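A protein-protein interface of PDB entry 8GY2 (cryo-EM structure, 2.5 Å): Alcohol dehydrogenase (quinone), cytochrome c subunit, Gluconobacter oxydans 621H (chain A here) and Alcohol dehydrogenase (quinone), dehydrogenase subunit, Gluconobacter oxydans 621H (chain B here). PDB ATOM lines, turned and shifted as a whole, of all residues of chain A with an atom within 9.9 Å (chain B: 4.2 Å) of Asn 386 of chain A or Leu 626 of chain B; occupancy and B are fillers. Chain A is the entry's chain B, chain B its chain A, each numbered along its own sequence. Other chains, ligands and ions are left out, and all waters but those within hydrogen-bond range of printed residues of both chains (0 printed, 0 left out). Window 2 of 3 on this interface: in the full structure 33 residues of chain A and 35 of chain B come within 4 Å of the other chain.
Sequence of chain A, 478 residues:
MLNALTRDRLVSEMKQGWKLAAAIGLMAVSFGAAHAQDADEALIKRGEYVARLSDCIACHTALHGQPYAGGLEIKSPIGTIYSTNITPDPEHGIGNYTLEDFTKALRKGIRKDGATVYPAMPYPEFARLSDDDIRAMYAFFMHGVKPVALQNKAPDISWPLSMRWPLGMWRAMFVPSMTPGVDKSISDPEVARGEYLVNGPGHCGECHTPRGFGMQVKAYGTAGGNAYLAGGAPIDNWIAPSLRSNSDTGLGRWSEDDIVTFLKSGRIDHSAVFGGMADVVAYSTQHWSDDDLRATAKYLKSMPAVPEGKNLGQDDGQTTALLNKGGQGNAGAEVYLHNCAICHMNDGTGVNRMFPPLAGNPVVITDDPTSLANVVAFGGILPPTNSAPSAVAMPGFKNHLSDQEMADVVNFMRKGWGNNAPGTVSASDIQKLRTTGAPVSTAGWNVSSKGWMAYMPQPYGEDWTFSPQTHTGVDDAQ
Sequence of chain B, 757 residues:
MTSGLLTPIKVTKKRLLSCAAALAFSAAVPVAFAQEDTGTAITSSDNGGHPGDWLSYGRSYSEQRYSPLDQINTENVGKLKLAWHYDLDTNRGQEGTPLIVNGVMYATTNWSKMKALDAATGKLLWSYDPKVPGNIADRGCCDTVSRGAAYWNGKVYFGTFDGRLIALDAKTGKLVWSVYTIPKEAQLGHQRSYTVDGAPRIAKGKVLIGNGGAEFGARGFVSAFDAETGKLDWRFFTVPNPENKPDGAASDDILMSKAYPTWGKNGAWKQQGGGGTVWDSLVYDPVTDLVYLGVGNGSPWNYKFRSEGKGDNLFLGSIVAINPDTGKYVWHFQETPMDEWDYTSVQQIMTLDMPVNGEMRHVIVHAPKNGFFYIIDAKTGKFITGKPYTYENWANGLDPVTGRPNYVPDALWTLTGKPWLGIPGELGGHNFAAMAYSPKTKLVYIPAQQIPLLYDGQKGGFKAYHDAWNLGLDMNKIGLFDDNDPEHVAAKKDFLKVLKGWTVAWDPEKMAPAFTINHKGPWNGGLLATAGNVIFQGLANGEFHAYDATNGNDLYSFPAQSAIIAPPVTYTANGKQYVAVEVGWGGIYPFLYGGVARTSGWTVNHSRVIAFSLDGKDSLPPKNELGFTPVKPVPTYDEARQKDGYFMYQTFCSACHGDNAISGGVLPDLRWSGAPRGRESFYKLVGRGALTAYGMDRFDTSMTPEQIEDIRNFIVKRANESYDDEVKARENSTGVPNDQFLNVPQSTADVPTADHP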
ATOM      1  N   THR A 261     -18.770  -1.689  28.834  1.00  0.00           N
ATOM      2  CA  THR A 261     -17.882  -0.586  28.484  1.00  0.00           C
ATOM      3  C   THR A 261     -16.544  -0.696  29.206  1.00  0.00           C
ATOM      4  O   THR A 261     -15.494  -0.406  28.622  1.00  0.00           O
ATOM      5  CB  THR A 261     -18.555   0.751  28.795  1.00  0.00           C
ATOM      6  OG1 THR A 261     -19.838   0.797  28.161  1.00  0.00           O
ATOM      7  CG2 THR A 261     -17.708   1.904  28.283  1.00  0.00           C
ATOM      8  N   LYS A 264     -14.566  -3.321  27.411  1.00  0.00           N
ATOM      9  CA  LYS A 264     -14.149  -2.928  26.070  1.00  0.00           C
ATOM     10  C   LYS A 264     -13.035  -1.886  26.103  1.00  0.00           C
ATOM     11  O   LYS A 264     -12.053  -2.000  25.364  1.00  0.00           O
ATOM     12  CB  LYS A 264     -15.347  -2.404  25.280  1.00  0.00           C
ATOM     13  CG  LYS A 264     -14.987  -1.840  23.918  1.00  0.00           C
ATOM     14  CD  LYS A 264     -15.969  -2.297  22.853  1.00  0.00           C
ATOM     15  CE  LYS A 264     -15.397  -3.440  22.031  1.00  0.00           C
ATOM     16  NZ  LYS A 264     -14.188  -3.024  21.270  1.00  0.00           N
ATOM     17  N   SER A 265     -13.164  -0.865  26.954  1.00  0.00           N
ATOM     18  CA  SER A 265     -12.239   0.259  26.942  1.00  0.00           C
ATOM     19  C   SER A 265     -11.563   0.541  28.275  1.00  0.00           C
ATOM     20  O   SER A 265     -10.519   1.200  28.283  1.00  0.00           O
ATOM     21  CB  SER A 265     -12.955   1.538  26.480  1.00  0.00           C
ATOM     22  OG  SER A 265     -14.285   1.580  26.964  1.00  0.00           O
ATOM     23  N   GLY A 266     -12.115   0.075  29.391  1.00  0.00           N
ATOM     24  CA  GLY A 266     -11.480   0.273  30.677  1.00  0.00           C
ATOM     25  C   GLY A 266     -11.760   1.595  31.352  1.00  0.00           C
ATOM     26  O   GLY A 266     -11.113   1.902  32.360  1.00  0.00           O
ATOM     27  N   ARG A 267     -12.698   2.390  30.840  1.00  0.00           N
ATOM     28  CA  ARG A 267     -12.985   3.705  31.407  1.00  0.00           C
ATOM     29  C   ARG A 267     -14.491   3.923  31.424  1.00  0.00           C
ATOM     30  O   ARG A 267     -15.096   4.172  30.378  1.00  0.00           O
ATOM     31  CB  ARG A 267     -12.287   4.811  30.616  1.00  0.00           C
ATOM     32  CG  ARG A 267     -10.792   4.888  30.851  1.00  0.00           C
ATOM     33  CD  ARG A 267     -10.132   5.872  29.906  1.00  0.00           C
ATOM     34  NE  ARG A 267     -10.311   7.248  30.347  1.00  0.00           N
ATOM     35  CZ  ARG A 267      -9.783   8.302  29.742  1.00  0.00           C
ATOM     36  NH1 ARG A 267      -9.028   8.174  28.663  1.00  0.00           N
ATOM     37  NH2 ARG A 267     -10.019   9.516  30.229  1.00  0.00           N
ATOM     38  N   ASP A 290     -18.782  -7.474  20.397  1.00  0.00           N
ATOM     39  CA  ASP A 290     -19.795  -6.861  21.248  1.00  0.00           C
ATOM     40  C   ASP A 290     -20.747  -7.906  21.813  1.00  0.00           C
ATOM     41  O   ASP A 290     -21.187  -7.800  22.963  1.00  0.00           O
ATOM     42  CB  ASP A 290     -20.564  -5.796  20.468  1.00  0.00           C
ATOM     43  CG  ASP A 290     -19.829  -4.473  20.411  1.00  0.00           C
ATOM     44  OD1 ASP A 290     -19.623  -3.861  21.480  1.00  0.00           O
ATOM     45  OD2 ASP A 290     -19.458  -4.044  19.298  1.00  0.00           O
ATOM     46  N   ARG A 353     -15.543   9.588  34.004  1.00  0.00           N
ATOM     47  CA  ARG A 353     -14.834   9.070  32.838  1.00  0.00           C
ATOM     48  C   ARG A 353     -13.448   9.682  32.657  1.00  0.00           C
ATOM     49  O   ARG A 353     -12.769   9.389  31.669  1.00  0.00           O
ATOM     50  CB  ARG A 353     -15.667   9.279  31.569  1.00  0.00           C
ATOM     51  CG  ARG A 353     -16.661   8.164  31.296  1.00  0.00           C
ATOM     52  CD  ARG A 353     -18.030   8.718  30.957  1.00  0.00           C
ATOM     53  NE  ARG A 353     -17.940   9.905  30.115  1.00  0.00           N
ATOM     54  CZ  ARG A 353     -18.614  11.026  30.327  1.00  0.00           C
ATOM     55  NH1 ARG A 353     -19.443  11.151  31.349  1.00  0.00           N
ATOM     56  NH2 ARG A 353     -18.451  12.047  29.492  1.00  0.00           N
ATOM     57  N   PRO A 383      -5.404   5.412  27.536  1.00  0.00           N
ATOM     58  CA  PRO A 383      -5.658   6.107  26.272  1.00  0.00           C
ATOM     59  C   PRO A 383      -7.074   6.649  26.224  1.00  0.00           C
ATOM     60  O   PRO A 383      -7.940   6.209  26.994  1.00  0.00           O
ATOM     61  CB  PRO A 383      -5.448   5.003  25.223  1.00  0.00           C
ATOM     62  CG  PRO A 383      -5.770   3.748  25.939  1.00  0.00           C
ATOM     63  CD  PRO A 383      -5.322   3.951  27.360  1.00  0.00           C
ATOM     64  N   PRO A 384      -7.353   7.607  25.340  1.00  0.00           N
ATOM     65  CA  PRO A 384      -8.719   8.118  25.234  1.00  0.00           C
ATOM     66  C   PRO A 384      -9.625   7.116  24.539  1.00  0.00           C
ATOM     67  O   PRO A 384      -9.183   6.306  23.720  1.00  0.00           O
ATOM     68  CB  PRO A 384      -8.567   9.399  24.404  1.00  0.00           C
ATOM     69  CG  PRO A 384      -7.140   9.436  23.931  1.00  0.00           C
ATOM     70  CD  PRO A 384      -6.487   8.141  24.277  1.00  0.00           C
ATOM     71  N   THR A 385     -10.905   7.178  24.877  1.00  0.00           N
ATOM     72  CA  THR A 385     -11.926   6.337  24.272  1.00  0.00           C
ATOM     73  C   THR A 385     -12.980   7.221  23.616  1.00  0.00           C
ATOM     74  O   THR A 385     -12.881   8.450  23.615  1.00  0.00           O
ATOM     75  CB  THR A 385     -12.563   5.407  25.310  1.00  0.00           C
ATOM     76  OG1 THR A 385     -13.564   6.121  26.043  1.00  0.00           O
ATOM     77  CG2 THR A 385     -11.513   4.884  26.278  1.00  0.00           C
ATOM     78  N   ASN A 386     -13.996   6.576  23.039  1.00  0.00           N
ATOM     79  CA  ASN A 386     -15.079   7.327  22.413  1.00  0.00           C
ATOM     80  C   ASN A 386     -15.859   8.133  23.443  1.00  0.00           C
ATOM     81  O   ASN A 386     -16.164   9.311  23.221  1.00  0.00           O
ATOM     82  CB  ASN A 386     -16.011   6.377  21.661  1.00  0.00           C
ATOM     83  CG  ASN A 386     -15.348   5.745  20.456  1.00  0.00           C
ATOM     84  OD1 ASN A 386     -14.470   6.340  19.833  1.00  0.00           O
ATOM     85  ND2 ASN A 386     -15.767   4.533  20.120  1.00  0.00           N
ATOM     86  N   SER A 387     -16.184   7.520  24.579  1.00  0.00           N
ATOM     87  CA  SER A 387     -16.942   8.186  25.628  1.00  0.00           C
ATOM     88  C   SER A 387     -16.059   8.808  26.699  1.00  0.00           C
ATOM     89  O   SER A 387     -16.556   9.604  27.503  1.00  0.00           O
ATOM     90  CB  SER A 387     -17.914   7.200  26.281  1.00  0.00           C
ATOM     91  OG  SER A 387     -17.215   6.190  26.987  1.00  0.00           O
ATOM     92  N   ALA A 388     -14.772   8.470  26.732  1.00  0.00           N
ATOM     93  CA  ALA A 388     -13.827   9.009  27.708  1.00  0.00           C
ATOM     94  C   ALA A 388     -12.629   9.564  26.953  1.00  0.00           C
ATOM     95  O   ALA A 388     -11.589   8.902  26.838  1.00  0.00           O
ATOM     96  CB  ALA A 388     -13.406   7.946  28.722  1.00  0.00           C
ATOM     97  N   PRO A 389     -12.739  10.778  26.423  1.00  0.00           N
ATOM     98  CA  PRO A 389     -11.616  11.371  25.689  1.00  0.00           C
ATOM     99  C   PRO A 389     -10.528  11.863  26.626  1.00  0.00           C
ATOM    100  O   PRO A 389     -10.585  11.603  27.832  1.00  0.00           O
ATOM    101  CB  PRO A 389     -12.266  12.526  24.920  1.00  0.00           C
ATOM    102  CG  PRO A 389     -13.548  12.828  25.646  1.00  0.00           C
ATOM    103  CD  PRO A 389     -13.825  11.745  26.651  1.00  0.00           C
ATOM    104  N   SER A 390      -9.534  12.570  26.087  1.00  0.00           N
ATOM    105  CA  SER A 390      -8.502  13.215  26.896  1.00  0.00           C
ATOM    106  C   SER A 390      -7.728  12.189  27.731  1.00  0.00           C
ATOM    107  O   SER A 390      -7.892  12.084  28.946  1.00  0.00           O
ATOM    108  CB  SER A 390      -9.107  14.304  27.789  1.00  0.00           C
ATOM    109  OG  SER A 390      -9.699  13.739  28.944  1.00  0.00           O
ATOM    110  N   ALA A 391      -6.919  11.399  27.020  1.00  0.00           N
ATOM    111  CA  ALA A 391      -6.027  10.409  27.622  1.00  0.00           C
ATOM    112  C   ALA A 391      -5.451  10.891  28.948  1.00  0.00           C
ATOM    113  O   ALA A 391      -4.942  12.009  29.050  1.00  0.00           O
ATOM    114  CB  ALA A 391      -4.883  10.091  26.658  1.00  0.00           C
ATOM    115  N   LYS A 450      -8.150  -1.188  17.269  1.00  0.00           N
ATOM    116  CA  LYS A 450      -8.872  -0.143  16.559  1.00  0.00           C
ATOM    117  C   LYS A 450      -8.943   1.157  17.344  1.00  0.00           C
ATOM    118  O   LYS A 450      -9.297   2.192  16.768  1.00  0.00           O
ATOM    119  CB  LYS A 450     -10.290  -0.615  16.227  1.00  0.00           C
ATOM    120  CG  LYS A 450     -10.362  -2.013  15.639  1.00  0.00           C
ATOM    121  CD  LYS A 450     -11.804  -2.430  15.403  1.00  0.00           C
ATOM    122  CE  LYS A 450     -11.963  -3.161  14.081  1.00  0.00           C
ATOM    123  NZ  LYS A 450     -13.012  -2.536  13.226  1.00  0.00           N
ATOM    124  N   GLY A 451      -8.617   1.132  18.632  1.00  0.00           N
ATOM    125  CA  GLY A 451      -8.669   2.313  19.463  1.00  0.00           C
ATOM    126  C   GLY A 451      -7.402   3.140  19.368  1.00  0.00           C
ATOM    127  O   GLY A 451      -6.523   2.912  18.534  1.00  0.00           O
ATOM    128  N   TRP A 452      -7.316   4.127  20.254  1.00  0.00           N
ATOM    129  CA  TRP A 452      -6.187   5.041  20.257  1.00  0.00           C
ATOM    130  C   TRP A 452      -5.020   4.474  21.058  1.00  0.00           C
ATOM    131  O   TRP A 452      -5.183   3.628  21.941  1.00  0.00           O
ATOM    132  CB  TRP A 452      -6.597   6.400  20.825  1.00  0.00           C
ATOM    133  CG  TRP A 452      -7.205   7.310  19.809  1.00  0.00           C
ATOM    134  CD1 TRP A 452      -6.626   7.754  18.657  1.00  0.00           C
ATOM    135  CD2 TRP A 452      -8.512   7.893  19.851  1.00  0.00           C
ATOM    136  NE1 TRP A 452      -7.490   8.576  17.978  1.00  0.00           N
ATOM    137  CE2 TRP A 452      -8.656   8.677  18.690  1.00  0.00           C
ATOM    138  CE3 TRP A 452      -9.575   7.828  20.756  1.00  0.00           C
ATOM    139  CZ2 TRP A 452      -9.819   9.390  18.411  1.00  0.00           C
ATOM    140  CZ3 TRP A 452     -10.728   8.535  20.477  1.00  0.00           C
ATOM    141  CH2 TRP A 452     -10.840   9.306  19.316  1.00  0.00           C
ATOM    142  N   TRP B 602     -16.642  13.246   6.901  1.00  0.00           N
ATOM    143  CA  TRP B 602     -16.333  12.853   8.268  1.00  0.00           C
ATOM    144  C   TRP B 602     -14.890  12.378   8.377  1.00  0.00           C
ATOM    145  O   TRP B 602     -14.389  11.655   7.511  1.00  0.00           O
ATOM    146  CB  TRP B 602     -17.280  11.750   8.735  1.00  0.00           C
ATOM    147  CG  TRP B 602     -16.967  11.248  10.109  1.00  0.00           C
ATOM    148  CD1 TRP B 602     -16.344  10.079  10.432  1.00  0.00           C
ATOM    149  CD2 TRP B 602     -17.255  11.905  11.348  1.00  0.00           C
ATOM    150  NE1 TRP B 602     -16.230   9.966  11.796  1.00  0.00           N
ATOM    151  CE2 TRP B 602     -16.783  11.074  12.381  1.00  0.00           C
ATOM    152  CE3 TRP B 602     -17.870  13.114  11.682  1.00  0.00           C
ATOM    153  CZ2 TRP B 602     -16.906  11.414  13.725  1.00  0.00           C
ATOM    154  CZ3 TRP B 602     -17.990  13.449  13.017  1.00  0.00           C
ATOM    155  CH2 TRP B 602     -17.511  12.602  14.021  1.00  0.00           C
ATOM    156  N   ASN B 624     -11.122   2.672  14.599  1.00  0.00           N
ATOM    157  CA  ASN B 624     -12.397   3.193  15.074  1.00  0.00           C
ATOM    158  C   ASN B 624     -12.556   4.638  14.619  1.00  0.00           C
ATOM    159  O   ASN B 624     -11.713   5.488  14.925  1.00  0.00           O
ATOM    160  CB  ASN B 624     -12.477   3.091  16.594  1.00  0.00           C
ATOM    161  CG  ASN B 624     -13.890   3.241  17.114  1.00  0.00           C
ATOM    162  OD1 ASN B 624     -14.136   3.973  18.072  1.00  0.00           O
ATOM    163  ND2 ASN B 624     -14.829   2.547  16.485  1.00  0.00           N
ATOM    164  N   GLU B 625     -13.638   4.918  13.893  1.00  0.00           N
ATOM    165  CA  GLU B 625     -13.889   6.243  13.338  1.00  0.00           C
ATOM    166  C   GLU B 625     -15.076   6.937  13.997  1.00  0.00           C
ATOM    167  O   GLU B 625     -15.612   7.899  13.439  1.00  0.00           O
ATOM    168  CB  GLU B 625     -14.103   6.150  11.828  1.00  0.00           C
ATOM    169  CG  GLU B 625     -13.141   5.209  11.125  1.00  0.00           C
ATOM    170  CD  GLU B 625     -12.227   5.928  10.155  1.00  0.00           C
ATOM    171  OE1 GLU B 625     -12.015   7.146  10.326  1.00  0.00           O
ATOM    172  OE2 GLU B 625     -11.719   5.273   9.222  1.00  0.00           O
ATOM    173  N   LEU B 626     -15.500   6.468  15.171  1.00  0.00           N
ATOM    174  CA  LEU B 626     -16.641   7.078  15.842  1.00  0.00           C
ATOM    175  C   LEU B 626     -16.301   8.426  16.462  1.00  0.00           C
ATOM    176  O   LEU B 626     -17.209   9.233  16.689  1.00  0.00           O
ATOM    177  CB  LEU B 626     -17.185   6.137  16.917  1.00  0.00           C
ATOM    178  CG  LEU B 626     -17.698   4.783  16.431  1.00  0.00           C
ATOM    179  CD1 LEU B 626     -18.311   4.006  17.581  1.00  0.00           C
ATOM    180  CD2 LEU B 626     -18.704   4.965  15.308  1.00  0.00           C
ATOM    181  N   GLY B 627     -15.026   8.690  16.737  1.00  0.00           N
ATOM    182  CA  GLY B 627     -14.662   9.957  17.348  1.00  0.00           C
ATOM    183  C   GLY B 627     -15.126  10.027  18.789  1.00  0.00           C
ATOM    184  O   GLY B 627     -15.105   9.036  19.525  1.00  0.00           O
ATOM    185  N   PHE B 628     -15.550  11.218  19.204  1.00  0.00           N
ATOM    186  CA  PHE B 628     -16.047  11.447  20.555  1.00  0.00           C
ATOM    187  C   PHE B 628     -17.571  11.424  20.519  1.00  0.00           C
ATOM    188  O   PHE B 628     -18.203  12.367  20.032  1.00  0.00           O
ATOM    189  CB  PHE B 628     -15.520  12.771  21.107  1.00  0.00           C
ATOM    190  CG  PHE B 628     -14.022  12.875  21.091  1.00  0.00           C
ATOM    191  CD1 PHE B 628     -13.238  11.822  21.528  1.00  0.00           C
ATOM    192  CD2 PHE B 628     -13.398  14.023  20.637  1.00  0.00           C
ATOM    193  CE1 PHE B 628     -11.861  11.911  21.512  1.00  0.00           C
ATOM    194  CE2 PHE B 628     -12.021  14.117  20.619  1.00  0.00           C
ATOM    195  CZ  PHE B 628     -11.252  13.061  21.059  1.00  0.00           C
ATOM    196  N   THR B 629     -18.156  10.344  21.033  1.00  0.00           N
ATOM    197  CA  THR B 629     -19.596  10.144  21.010  1.00  0.00           C
ATOM    198  C   THR B 629     -20.274  10.932  22.130  1.00  0.00           C
ATOM    199  O   THR B 629     -19.675  11.173  23.181  1.00  0.00           O
ATOM    200  CB  THR B 629     -19.926   8.663  21.150  1.00  0.00           C
ATOM    201  OG1 THR B 629     -19.536   8.206  22.451  1.00  0.00           O
ATOM    202  CG2 THR B 629     -19.191   7.855  20.094  1.00  0.00           C
ATOM    203  N   GLY B 735     -22.776   4.627  12.038  1.00  0.00           N
ATOM    204  CA  GLY B 735     -22.517   5.064  13.392  1.00  0.00           C
ATOM    205  C   GLY B 735     -21.930   6.453  13.524  1.00  0.00           C
ATOM    206  O   GLY B 735     -21.657   6.886  14.650  1.00  0.00           O
ATOM    207  N   VAL B 736     -21.728   7.158  12.420  1.00  0.00           N
ATOM    208  CA  VAL B 736     -21.206   8.522  12.443  1.00  0.00           C
ATOM    209  C   VAL B 736     -22.290   9.434  11.888  1.00  0.00           C
ATOM    210  O   VAL B 736     -23.201   8.974  11.176  1.00  0.00           O
ATOM    211  CB  VAL B 736     -19.883   8.643  11.651  1.00  0.00           C
ATOM    212  CG1 VAL B 736     -18.936   7.512  12.018  1.00  0.00           C
ATOM    213  CG2 VAL B 736     -20.150   8.665  10.156  1.00  0.00           C
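O of Thr 385 of chain A touches CD1 of Phe 628 of chain B, 3.98 Å away. CD1 of Leu 626 of chain B touches ND2 of Asn 386 of chain A, 3.6 Å away. Phe 628 of chain B touches Asn 386 of chain A (CA to O, 3.4 Å). Phe 628 of chain B touches Pro 389 of chain A. Trp 452 of chain A touches Phe 628 of chain B.
Of the 9 printed residues of chain B, 5 touch a printed residue of chain A. Hydrophobic or aromatic side chains of chain B that line the printed part of chain A: Leu 626 and Phe 628. Among the printed residues, no Asp or Glu carboxylate lies within 4 Å of a Lys or Arg side-chain nitrogen of the other chain.
Of the printed residues of chain B, Thr 385 of chain A touches Phe 628. Asn 386 of chain A touches just these residues of chain B: Asn 624 (2.7 Å), Leu 626 (3.6 Å), Gly 627 (2.8 Å), Phe 628 (3.4 Å) and Thr 629 (3.1 Å). Printed residues of chain B within 4 Å of Lys 450 of chain A: Asn 624 (2.9 Å). Of the printed residues of chain B, Trp 452 of chain A touches Phe 628. Leu 626 of chain B touches one residue of chain A. Of chain A, only Asn 386 (2.8 Å) comes within 4 Å of Gly 627 of chain B. Of the printed residues of chain A, Phe 628 of chain B touches Thr 385, Asn 386, Pro 389 and Trp 452. Thr 629 of chain B touches just one residue of chain A: Asn 386 (3.1 Å). No residue of chain A comes within 4 Å of Gly 735 of chain B. The nearest printed residue of chain B that does not touch Asn 386 of chain A is Glu 625 of chain B (5.9 Å). The nearest printed residue of chain B that does not touch Thr 385 of chain A is Gly 627 of chain B (4.7 Å).
O of Pro 389 of chain A lies within hydrogen-bond range of NH2 of Arg 267 of chain A (3.2 Å). The side-chain hydroxyl (OG1) of Thr 385 of chain A is in hydrogen-bond range of the backbone NH (N) of Ser 387 of chain A (3.3 Å). The backbone NH of Ala 388 of chain A lies within hydrogen-bond range of the side-chain hydroxyl of Thr 385 of chain A (2.7 Å).
OD1 of Asn 624 of chain B sits at hydrogen-bond distance from ND2 of Asn 386 of chain A (2.7 Å). O of Lys 450 of chain A lies within hydrogen-bond range of N of Asn 624 of chain B (2.9 Å). O of Gly 627 of chain B lies close to OD1 of Asn 386 of chain A, at 2.8 Å. The backbone carbonyl oxygen (O) of Asn 386 of chain A is in hydrogen-bond range of the backbone NH (N) of Thr 629 of chain B (3.1 Å).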
